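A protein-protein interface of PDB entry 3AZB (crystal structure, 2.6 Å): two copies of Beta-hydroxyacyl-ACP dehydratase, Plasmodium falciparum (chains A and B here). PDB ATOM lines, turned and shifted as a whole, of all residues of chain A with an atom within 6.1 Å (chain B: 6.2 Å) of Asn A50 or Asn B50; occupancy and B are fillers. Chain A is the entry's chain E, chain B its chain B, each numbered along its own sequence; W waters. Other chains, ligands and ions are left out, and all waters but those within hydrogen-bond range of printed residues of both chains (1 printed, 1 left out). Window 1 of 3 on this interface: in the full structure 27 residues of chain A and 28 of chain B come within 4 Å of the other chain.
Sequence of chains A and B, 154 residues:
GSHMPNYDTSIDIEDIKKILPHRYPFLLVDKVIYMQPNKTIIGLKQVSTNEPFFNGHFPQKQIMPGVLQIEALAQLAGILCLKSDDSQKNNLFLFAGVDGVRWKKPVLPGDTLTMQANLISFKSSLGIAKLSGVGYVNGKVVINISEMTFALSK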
ATOM      1  N   ARG A  23     -32.424 -18.117  -6.534  1.00  0.00           N
ATOM      2  CA  ARG A  23     -31.234 -17.942  -7.348  1.00  0.00           C
ATOM      3  C   ARG A  23     -30.867 -19.218  -8.116  1.00  0.00           C
ATOM      4  O   ARG A  23     -31.586 -20.219  -8.066  1.00  0.00           O
ATOM      5  CB  ARG A  23     -30.075 -17.429  -6.483  1.00  0.00           C
ATOM      6  CG  ARG A  23     -30.340 -16.062  -5.800  1.00  0.00           C
ATOM      7  CD  ARG A  23     -30.625 -14.971  -6.812  1.00  0.00           C
ATOM      8  NE  ARG A  23     -30.806 -13.647  -6.213  1.00  0.00           N
ATOM      9  CZ  ARG A  23     -31.983 -13.035  -6.051  1.00  0.00           C
ATOM     10  NH1 ARG A  23     -33.120 -13.604  -6.427  1.00  0.00           N
ATOM     11  NH2 ARG A  23     -32.031 -11.833  -5.525  1.00  0.00           N
ATOM     12  N   TYR A  24     -29.764 -19.167  -8.851  1.00  0.00           N
ATOM     13  CA  TYR A  24     -29.241 -20.337  -9.562  1.00  0.00           C
ATOM     14  C   TYR A  24     -28.802 -21.392  -8.537  1.00  0.00           C
ATOM     15  O   TYR A  24     -28.196 -21.053  -7.524  1.00  0.00           O
ATOM     16  CB  TYR A  24     -28.068 -19.910 -10.445  1.00  0.00           C
ATOM     17  CG  TYR A  24     -27.324 -21.028 -11.139  1.00  0.00           C
ATOM     18  CD1 TYR A  24     -27.652 -21.401 -12.429  1.00  0.00           C
ATOM     19  CD2 TYR A  24     -26.259 -21.692 -10.508  1.00  0.00           C
ATOM     20  CE1 TYR A  24     -26.955 -22.432 -13.075  1.00  0.00           C
ATOM     21  CE2 TYR A  24     -25.564 -22.726 -11.147  1.00  0.00           C
ATOM     22  CZ  TYR A  24     -25.915 -23.088 -12.429  1.00  0.00           C
ATOM     23  OH  TYR A  24     -25.235 -24.101 -13.090  1.00  0.00           O
ATOM     24  N   PRO A  25     -29.078 -22.674  -8.812  1.00  0.00           N
ATOM     25  CA  PRO A  25     -29.670 -23.204 -10.028  1.00  0.00           C
ATOM     26  C   PRO A  25     -31.158 -23.465  -9.902  1.00  0.00           C
ATOM     27  O   PRO A  25     -31.632 -24.432 -10.467  1.00  0.00           O
ATOM     28  CB  PRO A  25     -28.929 -24.536 -10.205  1.00  0.00           C
ATOM     29  CG  PRO A  25     -28.596 -24.986  -8.808  1.00  0.00           C
ATOM     30  CD  PRO A  25     -28.703 -23.767  -7.892  1.00  0.00           C
ATOM     31  N   PHE A  26     -31.883 -22.615  -9.177  1.00  0.00           N
ATOM     32  CA  PHE A  26     -33.305 -22.854  -8.914  1.00  0.00           C
ATOM     33  C   PHE A  26     -34.225 -21.650  -9.228  1.00  0.00           C
ATOM     34  O   PHE A  26     -35.322 -21.508  -8.682  1.00  0.00           O
ATOM     35  CB  PHE A  26     -33.512 -23.436  -7.493  1.00  0.00           C
ATOM     36  CG  PHE A  26     -34.470 -24.599  -7.460  1.00  0.00           C
ATOM     37  CD1 PHE A  26     -34.076 -25.856  -7.913  1.00  0.00           C
ATOM     38  CD2 PHE A  26     -35.775 -24.432  -7.027  1.00  0.00           C
ATOM     39  CE1 PHE A  26     -34.962 -26.922  -7.917  1.00  0.00           C
ATOM     40  CE2 PHE A  26     -36.659 -25.497  -7.022  1.00  0.00           C
ATOM     41  CZ  PHE A  26     -36.257 -26.739  -7.474  1.00  0.00           C
ATOM     42  N   LEU A  27     -33.771 -20.791 -10.131  1.00  0.00           N
ATOM     43  CA  LEU A  27     -34.621 -19.741 -10.697  1.00  0.00           C
ATOM     44  C   LEU A  27     -35.038 -20.203 -12.079  1.00  0.00           C
ATOM     45  O   LEU A  27     -34.201 -20.300 -12.977  1.00  0.00           O
ATOM     46  CB  LEU A  27     -33.885 -18.402 -10.787  1.00  0.00           C
ATOM     47  CG  LEU A  27     -34.605 -17.188 -11.395  1.00  0.00           C
ATOM     48  CD1 LEU A  27     -35.865 -16.803 -10.611  1.00  0.00           C
ATOM     49  CD2 LEU A  27     -33.659 -16.014 -11.427  1.00  0.00           C
ATOM     50  N   LEU A  28     -36.334 -20.476 -12.238  1.00  0.00           N
ATOM     51  CA  LEU A  28     -36.864 -21.080 -13.457  1.00  0.00           C
ATOM     52  C   LEU A  28     -37.823 -20.194 -14.254  1.00  0.00           C
ATOM     53  O   LEU A  28     -38.686 -20.701 -14.983  1.00  0.00           O
ATOM     54  CB  LEU A  28     -37.555 -22.390 -13.114  1.00  0.00           C
ATOM     55  CG  LEU A  28     -36.704 -23.444 -12.416  1.00  0.00           C
ATOM     56  CD1 LEU A  28     -37.554 -24.651 -12.071  1.00  0.00           C
ATOM     57  CD2 LEU A  28     -35.534 -23.858 -13.262  1.00  0.00           C
ATOM     58  N   ASP A  30     -37.503 -16.986 -16.863  1.00  0.00           N
ATOM     59  CA  ASP A  30     -36.557 -16.177 -17.621  1.00  0.00           C
ATOM     60  C   ASP A  30     -37.043 -14.756 -17.898  1.00  0.00           C
ATOM     61  O   ASP A  30     -36.252 -13.819 -17.825  1.00  0.00           O
ATOM     62  CB  ASP A  30     -36.162 -16.890 -18.906  1.00  0.00           C
ATOM     63  CG  ASP A  30     -35.194 -18.029 -18.659  1.00  0.00           C
ATOM     64  OD1 ASP A  30     -34.365 -17.926 -17.750  1.00  0.00           O
ATOM     65  OD2 ASP A  30     -35.241 -19.032 -19.380  1.00  0.00           O
ATOM     66  N   LYS A  45     -39.853 -19.628 -19.885  1.00  0.00           N
ATOM     67  CA  LYS A  45     -38.583 -20.220 -19.476  1.00  0.00           C
ATOM     68  C   LYS A  45     -37.954 -20.850 -20.713  1.00  0.00           C
ATOM     69  O   LYS A  45     -38.549 -21.712 -21.342  1.00  0.00           O
ATOM     70  CB  LYS A  45     -38.813 -21.266 -18.370  1.00  0.00           C
ATOM     71  CG  LYS A  45     -37.553 -21.855 -17.737  1.00  0.00           C
ATOM     72  CD  LYS A  45     -37.119 -23.137 -18.472  1.00  0.00           C
ATOM     73  CE  LYS A  45     -35.877 -23.755 -17.862  1.00  0.00           C
ATOM     74  NZ  LYS A  45     -34.808 -22.758 -17.654  1.00  0.00           N
ATOM     75  N   SER A  48     -32.678 -24.808 -22.372  1.00  0.00           N
ATOM     76  CA  SER A  48     -31.425 -25.081 -23.055  1.00  0.00           C
ATOM     77  C   SER A  48     -30.738 -26.319 -22.498  1.00  0.00           C
ATOM     78  O   SER A  48     -30.915 -26.673 -21.317  1.00  0.00           O
ATOM     79  CB  SER A  48     -30.478 -23.906 -22.898  1.00  0.00           C
ATOM     80  OG  SER A  48     -29.170 -24.327 -23.240  1.00  0.00           O
ATOM     81  N   THR A  49     -29.949 -26.972 -23.351  1.00  0.00           N
ATOM     82  CA  THR A  49     -29.082 -28.083 -22.928  1.00  0.00           C
ATOM     83  C   THR A  49     -28.058 -27.584 -21.898  1.00  0.00           C
ATOM     84  O   THR A  49     -27.549 -28.366 -21.100  1.00  0.00           O
ATOM     85  CB  THR A  49     -28.361 -28.743 -24.129  1.00  0.00           C
ATOM     86  OG1 THR A  49     -27.885 -30.039 -23.754  1.00  0.00           O
ATOM     87  CG2 THR A  49     -27.187 -27.887 -24.626  1.00  0.00           C
ATOM     88  N   ASN A  50     -27.786 -26.279 -21.906  1.00  0.00           N
ATOM     89  CA  ASN A  50     -26.861 -25.695 -20.940  1.00  0.00           C
ATOM     90  C   ASN A  50     -27.464 -25.393 -19.552  1.00  0.00           C
ATOM     91  O   ASN A  50     -27.217 -24.335 -18.982  1.00  0.00           O
ATOM     92  CB  ASN A  50     -26.168 -24.443 -21.502  1.00  0.00           C
ATOM     93  CG  ASN A  50     -24.714 -24.318 -21.019  1.00  0.00           C
ATOM     94  OD1 ASN A  50     -23.947 -25.296 -21.048  1.00  0.00           O
ATOM     95  ND2 ASN A  50     -24.330 -23.121 -20.577  1.00  0.00           N
ATOM     96  N   GLU A  51     -28.238 -26.332 -19.018  1.00  0.00           N
ATOM     97  CA  GLU A  51     -28.778 -26.247 -17.663  1.00  0.00           C
ATOM     98  C   GLU A  51     -28.280 -27.435 -16.856  1.00  0.00           C
ATOM     99  O   GLU A  51     -28.239 -28.558 -17.382  1.00  0.00           O
ATOM    100  CB  GLU A  51     -30.307 -26.225 -17.684  1.00  0.00           C
ATOM    101  CG  GLU A  51     -30.841 -25.060 -18.486  1.00  0.00           C
ATOM    102  CD  GLU A  51     -32.328 -24.878 -18.401  1.00  0.00           C
ATOM    103  OE1 GLU A  51     -32.865 -24.716 -17.291  1.00  0.00           O
ATOM    104  OE2 GLU A  51     -32.957 -24.861 -19.470  1.00  0.00           O
ATOM    105  N   PRO A  52     -27.903 -27.194 -15.576  1.00  0.00           N
ATOM    106  CA  PRO A  52     -27.245 -28.200 -14.734  1.00  0.00           C
ATOM    107  C   PRO A  52     -28.041 -29.478 -14.535  1.00  0.00           C
ATOM    108  O   PRO A  52     -27.439 -30.541 -14.371  1.00  0.00           O
ATOM    109  CB  PRO A  52     -27.047 -27.479 -13.387  1.00  0.00           C
ATOM    110  CG  PRO A  52     -27.908 -26.260 -13.438  1.00  0.00           C
ATOM    111  CD  PRO A  52     -28.064 -25.905 -14.872  1.00  0.00           C
ATOM    112  N   PHE A  53     -29.367 -29.392 -14.555  1.00  0.00           N
ATOM    113  CA  PHE A  53     -30.186 -30.577 -14.291  1.00  0.00           C
ATOM    114  C   PHE A  53     -30.194 -31.601 -15.425  1.00  0.00           C
ATOM    115  O   PHE A  53     -30.482 -32.776 -15.195  1.00  0.00           O
ATOM    116  CB  PHE A  53     -31.626 -30.198 -13.895  1.00  0.00           C
ATOM    117  CG  PHE A  53     -32.371 -29.437 -14.953  1.00  0.00           C
ATOM    118  CD1 PHE A  53     -32.983 -30.097 -16.017  1.00  0.00           C
ATOM    119  CD2 PHE A  53     -32.470 -28.072 -14.884  1.00  0.00           C
ATOM    120  CE1 PHE A  53     -33.673 -29.398 -16.998  1.00  0.00           C
ATOM    121  CE2 PHE A  53     -33.162 -27.362 -15.863  1.00  0.00           C
ATOM    122  CZ  PHE A  53     -33.755 -28.029 -16.924  1.00  0.00           C
ATOM    123  N   PHE A  54     -29.880 -31.163 -16.643  1.00  0.00           N
ATOM    124  CA  PHE A  54     -30.046 -32.048 -17.807  1.00  0.00           C
ATOM    125  C   PHE A  54     -29.152 -33.288 -17.846  1.00  0.00           C
ATOM    126  O   PHE A  54     -29.621 -34.351 -18.250  1.00  0.00           O
ATOM    127  CB  PHE A  54     -29.997 -31.283 -19.129  1.00  0.00           C
ATOM    128  CG  PHE A  54     -31.339 -30.817 -19.586  1.00  0.00           C
ATOM    129  CD1 PHE A  54     -32.386 -31.723 -19.719  1.00  0.00           C
ATOM    130  CD2 PHE A  54     -31.562 -29.485 -19.864  1.00  0.00           C
ATOM    131  CE1 PHE A  54     -33.633 -31.306 -20.129  1.00  0.00           C
ATOM    132  CE2 PHE A  54     -32.812 -29.044 -20.276  1.00  0.00           C
ATOM    133  CZ  PHE A  54     -33.849 -29.947 -20.409  1.00  0.00           C
ATOM    134  N   LEU A  68     -39.969 -29.745 -12.270  1.00  0.00           N
ATOM    135  CA  LEU A  68     -39.289 -28.480 -12.529  1.00  0.00           C
ATOM    136  C   LEU A  68     -40.162 -27.534 -13.320  1.00  0.00           C
ATOM    137  O   LEU A  68     -39.903 -26.322 -13.348  1.00  0.00           O
ATOM    138  CB  LEU A  68     -37.941 -28.686 -13.236  1.00  0.00           C
ATOM    139  CG  LEU A  68     -36.774 -29.167 -12.366  1.00  0.00           C
ATOM    140  CD1 LEU A  68     -35.511 -29.047 -13.167  1.00  0.00           C
ATOM    141  CD2 LEU A  68     -36.646 -28.371 -11.061  1.00  0.00           C
ATOM    142  N   ARG B  23     -19.959 -31.506 -24.550  1.00  0.00           N
ATOM    143  CA  ARG B  23     -20.978 -31.782 -23.546  1.00  0.00           C
ATOM    144  C   ARG B  23     -21.121 -30.574 -22.625  1.00  0.00           C
ATOM    145  O   ARG B  23     -20.546 -29.505 -22.906  1.00  0.00           O
ATOM    146  CB  ARG B  23     -20.632 -33.049 -22.752  1.00  0.00           C
ATOM    147  CG  ARG B  23     -20.659 -34.357 -23.541  1.00  0.00           C
ATOM    148  CD  ARG B  23     -22.013 -34.626 -24.195  1.00  0.00           C
ATOM    149  NE  ARG B  23     -22.045 -35.883 -24.947  1.00  0.00           N
ATOM    150  CZ  ARG B  23     -21.591 -36.052 -26.197  1.00  0.00           C
ATOM    151  NH1 ARG B  23     -21.051 -35.035 -26.891  1.00  0.00           N
ATOM    152  NH2 ARG B  23     -21.677 -37.255 -26.761  1.00  0.00           N
ATOM    153  N   TYR B  24     -21.895 -30.733 -21.549  1.00  0.00           N
ATOM    154  CA  TYR B  24     -22.095 -29.685 -20.551  1.00  0.00           C
ATOM    155  C   TYR B  24     -20.770 -29.409 -19.821  1.00  0.00           C
ATOM    156  O   TYR B  24     -20.002 -30.343 -19.564  1.00  0.00           O
ATOM    157  CB  TYR B  24     -23.192 -30.133 -19.573  1.00  0.00           C
ATOM    158  CG  TYR B  24     -23.528 -29.163 -18.451  1.00  0.00           C
ATOM    159  CD1 TYR B  24     -24.591 -28.265 -18.571  1.00  0.00           C
ATOM    160  CD2 TYR B  24     -22.797 -29.161 -17.260  1.00  0.00           C
ATOM    161  CE1 TYR B  24     -24.910 -27.369 -17.533  1.00  0.00           C
ATOM    162  CE2 TYR B  24     -23.099 -28.276 -16.227  1.00  0.00           C
ATOM    163  CZ  TYR B  24     -24.158 -27.376 -16.370  1.00  0.00           C
ATOM    164  OH  TYR B  24     -24.476 -26.516 -15.349  1.00  0.00           O
ATOM    165  N   PRO B  25     -20.478 -28.133 -19.494  1.00  0.00           N
ATOM    166  CA  PRO B  25     -21.257 -26.911 -19.734  1.00  0.00           C
ATOM    167  C   PRO B  25     -20.860 -26.199 -21.013  1.00  0.00           C
ATOM    168  O   PRO B  25     -20.780 -24.974 -21.017  1.00  0.00           O
ATOM    169  CB  PRO B  25     -20.858 -26.018 -18.548  1.00  0.00           C
ATOM    170  CG  PRO B  25     -19.415 -26.403 -18.268  1.00  0.00           C
ATOM    171  CD  PRO B  25     -19.237 -27.838 -18.748  1.00  0.00           C
ATOM    172  N   PHE B  26     -20.582 -26.935 -22.082  1.00  0.00           N
ATOM    173  CA  PHE B  26     -20.022 -26.274 -23.265  1.00  0.00           C
ATOM    174  C   PHE B  26     -20.579 -26.786 -24.593  1.00  0.00           C
ATOM    175  O   PHE B  26     -19.930 -26.667 -25.638  1.00  0.00           O
ATOM    176  CB  PHE B  26     -18.485 -26.301 -23.230  1.00  0.00           C
ATOM    177  CG  PHE B  26     -17.846 -24.983 -23.595  1.00  0.00           C
ATOM    178  CD1 PHE B  26     -17.761 -23.958 -22.668  1.00  0.00           C
ATOM    179  CD2 PHE B  26     -17.321 -24.771 -24.861  1.00  0.00           C
ATOM    180  CE1 PHE B  26     -17.164 -22.739 -22.983  1.00  0.00           C
ATOM    181  CE2 PHE B  26     -16.717 -23.566 -25.184  1.00  0.00           C
ATOM    182  CZ  PHE B  26     -16.650 -22.541 -24.243  1.00  0.00           C
ATOM    183  N   LEU B  27     -21.772 -27.368 -24.540  1.00  0.00           N
ATOM    184  CA  LEU B  27     -22.602 -27.541 -25.724  1.00  0.00           C
ATOM    185  C   LEU B  27     -23.534 -26.329 -25.837  1.00  0.00           C
ATOM    186  O   LEU B  27     -24.354 -26.070 -24.942  1.00  0.00           O
ATOM    187  CB  LEU B  27     -23.412 -28.830 -25.617  1.00  0.00           C
ATOM    188  CG  LEU B  27     -24.288 -29.327 -26.759  1.00  0.00           C
ATOM    189  CD1 LEU B  27     -23.469 -29.587 -28.017  1.00  0.00           C
ATOM    190  CD2 LEU B  27     -24.983 -30.601 -26.321  1.00  0.00           C
ATOM    191  N   LEU B  28     -23.392 -25.589 -26.934  1.00  0.00           N
ATOM    192  CA  LEU B  28     -24.154 -24.357 -27.154  1.00  0.00           C
ATOM    193  C   LEU B  28     -25.069 -24.399 -28.387  1.00  0.00           C
ATOM    194  O   LEU B  28     -25.341 -23.370 -29.012  1.00  0.00           O
ATOM    195  CB  LEU B  28     -23.225 -23.125 -27.165  1.00  0.00           C
ATOM    196  CG  LEU B  28     -22.562 -22.881 -25.804  1.00  0.00           C
ATOM    197  CD1 LEU B  28     -21.391 -21.917 -25.890  1.00  0.00           C
ATOM    198  CD2 LEU B  28     -23.576 -22.417 -24.751  1.00  0.00           C
ATOM    199  N   ASP B  30     -28.897 -26.088 -29.169  1.00  0.00           N
ATOM    200  CA  ASP B  30     -30.050 -26.807 -28.648  1.00  0.00           C
ATOM    201  C   ASP B  30     -30.852 -27.539 -29.705  1.00  0.00           C
ATOM    202  O   ASP B  30     -31.418 -28.593 -29.447  1.00  0.00           O
ATOM    203  CB  ASP B  30     -30.961 -25.870 -27.870  1.00  0.00           C
ATOM    204  CG  ASP B  30     -30.360 -25.421 -26.568  1.00  0.00           C
ATOM    205  OD1 ASP B  30     -29.523 -26.143 -25.986  1.00  0.00           O
ATOM    206  OD2 ASP B  30     -30.745 -24.330 -26.124  1.00  0.00           O
ATOM    207  N   LYS B  45     -30.235 -21.671 -30.023  1.00  0.00           N
ATOM    208  CA  LYS B  45     -29.680 -21.873 -28.688  1.00  0.00           C
ATOM    209  C   LYS B  45     -30.525 -21.008 -27.759  1.00  0.00           C
ATOM    210  O   LYS B  45     -30.569 -19.765 -27.896  1.00  0.00           O
ATOM    211  CB  LYS B  45     -28.192 -21.480 -28.633  1.00  0.00           C
ATOM    212  CG  LYS B  45     -27.489 -21.713 -27.281  1.00  0.00           C
ATOM    213  CD  LYS B  45     -27.558 -20.484 -26.360  1.00  0.00           C
ATOM    214  CE  LYS B  45     -27.177 -20.804 -24.884  1.00  0.00           C
ATOM    215  NZ  LYS B  45     -27.929 -21.963 -24.311  1.00  0.00           N
ATOM    216  N   GLN B  46     -31.224 -21.672 -26.842  1.00  0.00           N
ATOM    217  CA  GLN B  46     -32.143 -20.989 -25.955  1.00  0.00           C
ATOM    218  C   GLN B  46     -31.361 -20.418 -24.779  1.00  0.00           C
ATOM    219  O   GLN B  46     -30.540 -21.093 -24.170  1.00  0.00           O
ATOM    220  CB  GLN B  46     -33.281 -21.927 -25.537  1.00  0.00           C
ATOM    221  CG  GLN B  46     -34.098 -22.516 -26.725  1.00  0.00           C
ATOM    222  CD  GLN B  46     -35.091 -21.518 -27.367  1.00  0.00           C
ATOM    223  OE1 GLN B  46     -35.045 -20.312 -27.127  1.00  0.00           O
ATOM    224  NE2 GLN B  46     -36.005 -22.039 -28.166  1.00  0.00           N
ATOM    225  N   SER B  48     -31.423 -19.156 -21.240  1.00  0.00           N
ATOM    226  CA  SER B  48     -32.134 -19.167 -19.962  1.00  0.00           C
ATOM    227  C   SER B  48     -31.240 -18.674 -18.827  1.00  0.00           C
ATOM    228  O   SER B  48     -30.039 -18.923 -18.849  1.00  0.00           O
ATOM    229  CB  SER B  48     -32.608 -20.592 -19.660  1.00  0.00           C
ATOM    230  OG  SER B  48     -33.156 -20.708 -18.348  1.00  0.00           O
ATOM    231  N   THR B  49     -31.817 -17.996 -17.834  1.00  0.00           N
ATOM    232  CA  THR B  49     -31.117 -17.656 -16.575  1.00  0.00           C
ATOM    233  C   THR B  49     -30.534 -18.863 -15.825  1.00  0.00           C
ATOM    234  O   THR B  49     -29.704 -18.706 -14.924  1.00  0.00           O
ATOM    235  CB  THR B  49     -32.086 -16.962 -15.530  1.00  0.00           C
ATOM    236  OG1 THR B  49     -31.342 -16.235 -14.533  1.00  0.00           O
ATOM    237  CG2 THR B  49     -33.008 -17.985 -14.828  1.00  0.00           C
ATOM    238  N   ASN B  50     -30.981 -20.065 -16.191  1.00  0.00           N
ATOM    239  CA  ASN B  50     -30.600 -21.261 -15.458  1.00  0.00           C
ATOM    240  C   ASN B  50     -29.376 -21.917 -16.050  1.00  0.00           C
ATOM    241  O   ASN B  50     -29.294 -23.145 -16.106  1.00  0.00           O
ATOM    242  CB  ASN B  50     -31.728 -22.273 -15.300  1.00  0.00           C
ATOM    243  CG  ASN B  50     -31.461 -23.253 -14.167  1.00  0.00           C
ATOM    244  OD1 ASN B  50     -30.927 -22.873 -13.112  1.00  0.00           O
ATOM    245  ND2 ASN B  50     -31.822 -24.531 -14.384  1.00  0.00           N
ATOM    246  N   GLU B  51     -28.425 -21.092 -16.481  1.00  0.00           N
ATOM    247  CA  GLU B  51     -27.206 -21.577 -17.121  1.00  0.00           C
ATOM    248  C   GLU B  51     -26.017 -21.164 -16.296  1.00  0.00           C
ATOM    249  O   GLU B  51     -26.019 -20.076 -15.727  1.00  0.00           O
ATOM    250  CB  GLU B  51     -27.074 -21.021 -18.546  1.00  0.00           C
ATOM    251  CG  GLU B  51     -28.171 -21.446 -19.485  1.00  0.00           C
ATOM    252  CD  GLU B  51     -27.912 -21.019 -20.935  1.00  0.00           C
ATOM    253  OE1 GLU B  51     -26.894 -21.471 -21.527  1.00  0.00           O
ATOM    254  OE2 GLU B  51     -28.747 -20.250 -21.473  1.00  0.00           O
ATOM    255  N   PRO B  52     -24.977 -22.012 -16.258  1.00  0.00           N
ATOM    256  CA  PRO B  52     -23.921 -21.831 -15.267  1.00  0.00           C
ATOM    257  C   PRO B  52     -23.094 -20.569 -15.415  1.00  0.00           C
ATOM    258  O   PRO B  52     -22.534 -20.111 -14.438  1.00  0.00           O
ATOM    259  CB  PRO B  52     -23.050 -23.083 -15.442  1.00  0.00           C
ATOM    260  CG  PRO B  52     -23.395 -23.629 -16.730  1.00  0.00           C
ATOM    261  CD  PRO B  52     -24.790 -23.247 -17.040  1.00  0.00           C
ATOM    262  N   PHE B  53     -23.004 -20.013 -16.617  1.00  0.00           N
ATOM    263  CA  PHE B  53     -22.159 -18.823 -16.850  1.00  0.00           C
ATOM    264  C   PHE B  53     -22.781 -17.527 -16.338  1.00  0.00           C
ATOM    265  O   PHE B  53     -22.083 -16.535 -16.095  1.00  0.00           O
ATOM    266  CB  PHE B  53     -21.785 -18.680 -18.334  1.00  0.00           C
ATOM    267  CG  PHE B  53     -22.964 -18.567 -19.271  1.00  0.00           C
ATOM    268  CD1 PHE B  53     -23.497 -17.331 -19.593  1.00  0.00           C
ATOM    269  CD2 PHE B  53     -23.511 -19.706 -19.863  1.00  0.00           C
ATOM    270  CE1 PHE B  53     -24.599 -17.226 -20.477  1.00  0.00           C
ATOM    271  CE2 PHE B  53     -24.592 -19.615 -20.756  1.00  0.00           C
ATOM    272  CZ  PHE B  53     -25.138 -18.363 -21.063  1.00  0.00           C
ATOM    273  N   PHE B  54     -24.097 -17.543 -16.174  1.00  0.00           N
ATOM    274  CA  PHE B  54     -24.833 -16.319 -15.912  1.00  0.00           C
ATOM    275  C   PHE B  54     -24.518 -15.664 -14.576  1.00  0.00           C
ATOM    276  O   PHE B  54     -24.542 -14.444 -14.492  1.00  0.00           O
ATOM    277  CB  PHE B  54     -26.342 -16.505 -16.144  1.00  0.00           C
ATOM    278  CG  PHE B  54     -26.789 -16.173 -17.561  1.00  0.00           C
ATOM    279  CD1 PHE B  54     -26.387 -14.994 -18.173  1.00  0.00           C
ATOM    280  CD2 PHE B  54     -27.624 -17.028 -18.268  1.00  0.00           C
ATOM    281  CE1 PHE B  54     -26.797 -14.663 -19.473  1.00  0.00           C
ATOM    282  CE2 PHE B  54     -28.042 -16.696 -19.576  1.00  0.00           C
ATOM    283  CZ  PHE B  54     -27.614 -15.504 -20.172  1.00  0.00           C
ATOM    284  N   LEU B  68     -19.185 -16.700 -26.102  1.00  0.00           N
ATOM    285  CA  LEU B  68     -20.032 -17.889 -26.102  1.00  0.00           C
ATOM    286  C   LEU B  68     -21.034 -17.874 -27.233  1.00  0.00           C
ATOM    287  O   LEU B  68     -21.581 -18.915 -27.577  1.00  0.00           O
ATOM    288  CB  LEU B  68     -20.784 -18.053 -24.773  1.00  0.00           C
ATOM    289  CG  LEU B  68     -19.994 -18.434 -23.523  1.00  0.00           C
ATOM    290  CD1 LEU B  68     -20.936 -18.554 -22.335  1.00  0.00           C
ATOM    291  CD2 LEU B  68     -19.209 -19.737 -23.753  1.00  0.00           C
HETATM  292  O   HOH W   1     -27.214 -24.229 -25.346  1.00  0.00           O
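OH of Tyr B24 sits at hydrogen-bond distance from OH of Tyr A24, at 3.4 Å. The backbone carbonyl oxygen (O) of Pro B25 sits close to the side-chain amide oxygen (OD1) of Asn A50, at 3.2 Å. OG of Ser A48 sits close to OD2 of Asp B30, at 3.3 Å. OD1 of Asp B30 sits at hydrogen-bond distance from N of Thr A49 (2.8 Å). The side-chain amino group (NZ) of Lys B45 is in hydrogen-bond range of the side-chain hydroxyl (OG) of Ser A48. OG of Ser B48 lies within hydrogen-bond range of OD2 of Asp A30 (2.9 Å). OG of Ser B48 is in hydrogen-bond range of NZ of Lys A45 (2.7 Å). OD1 of Asp A30 lies within hydrogen-bond range of N of Thr B49. The side-chain amide oxygen (OD1) of Asn B50 lies close to the backbone carbonyl oxygen (O) of Pro A25, 3.2 Å away. OE1 of Glu A51 sits at hydrogen-bond distance from ND2 of Asn B50 (3.1 Å). OE1 of Glu B51 sits close to ND2 of Asn A50, at 3.2 Å.
OD2 of Asp B30 sits at hydrogen-bond distance from N of Gln B46, 2.8 Å away. The side-chain carboxylate (OE1) of Glu B51 lies within salt-bridge range of the side-chain amino group (NZ) of Lys B45. The side-chain hydroxyl (OG) of Ser B48 lies close to the backbone NH (N) of Asn B50 (3.1 Å). The backbone NH of Ser B48 sits at hydrogen-bond distance from the side-chain carboxylate of Glu B51 (2.9 Å). The side-chain amino group (NZ) of Lys A45 is in salt-bridge range of the side-chain carboxylate (OE1) of Glu A51, at 2.8 Å. The backbone NH of Ser A48 lies within hydrogen-bond range of the side-chain carboxylate of Glu A51, 2.9 Å away.
Tyr A24 touches Asn B50. Asn B50 touches Leu A27. ND2 of Asn B50 touches CD2 of Leu A28, 3.9 Å away. NZ of Lys A45 touches CB of Asn B50 (3.9 Å). O of Thr A49 touches CD1 of Tyr B24 (3.9 Å). CG2 of Thr A49 touches O of Leu B27, at 3.4 Å. C of Asn A50 touches CE1 of Tyr B24, at 3.8 Å. Leu B27 touches Asn A50. ND2 of Asn A50 touches CE2 of Phe B53, at 3.5 Å. CD of Pro A52 touches O of Asn B50, 3.3 Å away.
Of the printed residues of chain B, Asp A30 touches Ser B48 and Thr B49. Of the printed residues of chain B, Lys A45 touches Ser B48 and Asn B50. Leu B28 touches none of the printed residues of chain A. Asn B50 touches just these residues of chain A: Tyr A24, Pro A25, Leu A27, Leu A28, Lys A45, Asn A50, Glu A51, Pro A52 and Phe A53. The nearest printed residue of chain B that does not touch Asn A50 is Lys B45 (4.1 Å). The nearest printed residue of chain A that does not touch Pro B52 is Pro A52 (4.7 Å).
Hydrophobic or aromatic side chains of chain B within 4 Å of the printed part of chain A: Tyr B24, Leu B27, Pro B52 and Phe B53. Of the 16 printed residues of chain A, 12 touch a printed residue of chain B. Among the printed residues, 31 pairs touch across the chains.
Leu A27 touches Thr B49, and with the chains exchanged Thr A49 touches Leu B27. Asp A30 touches Thr B49, and with the chains exchanged Thr A49 touches Asp B30. Lys A45 touches Ser B48, and with the chains exchanged Ser A48 touches Lys B45. Thr A49 touches Tyr B24, but with the chains exchanged Tyr A24 does not touch Thr B49 (4.2 Å). 16 positions are printed for both chains. Of the 31 pairs that touch across the chains among the printed residues, 26 have their exchanged pair printed and touching as well.
Water W1 lies within hydrogen-bond range of the side-chain amino group (NZ) of Lys B45 (2.6 Å), the side-chain hydroxyl (OG) of Ser A48 (2.9 Å), the side-chain carboxylate (OD1) of Asp B30 (3.1 Å) and the backbone carbonyl oxygen (O) of Leu B27 (3.4 Å).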
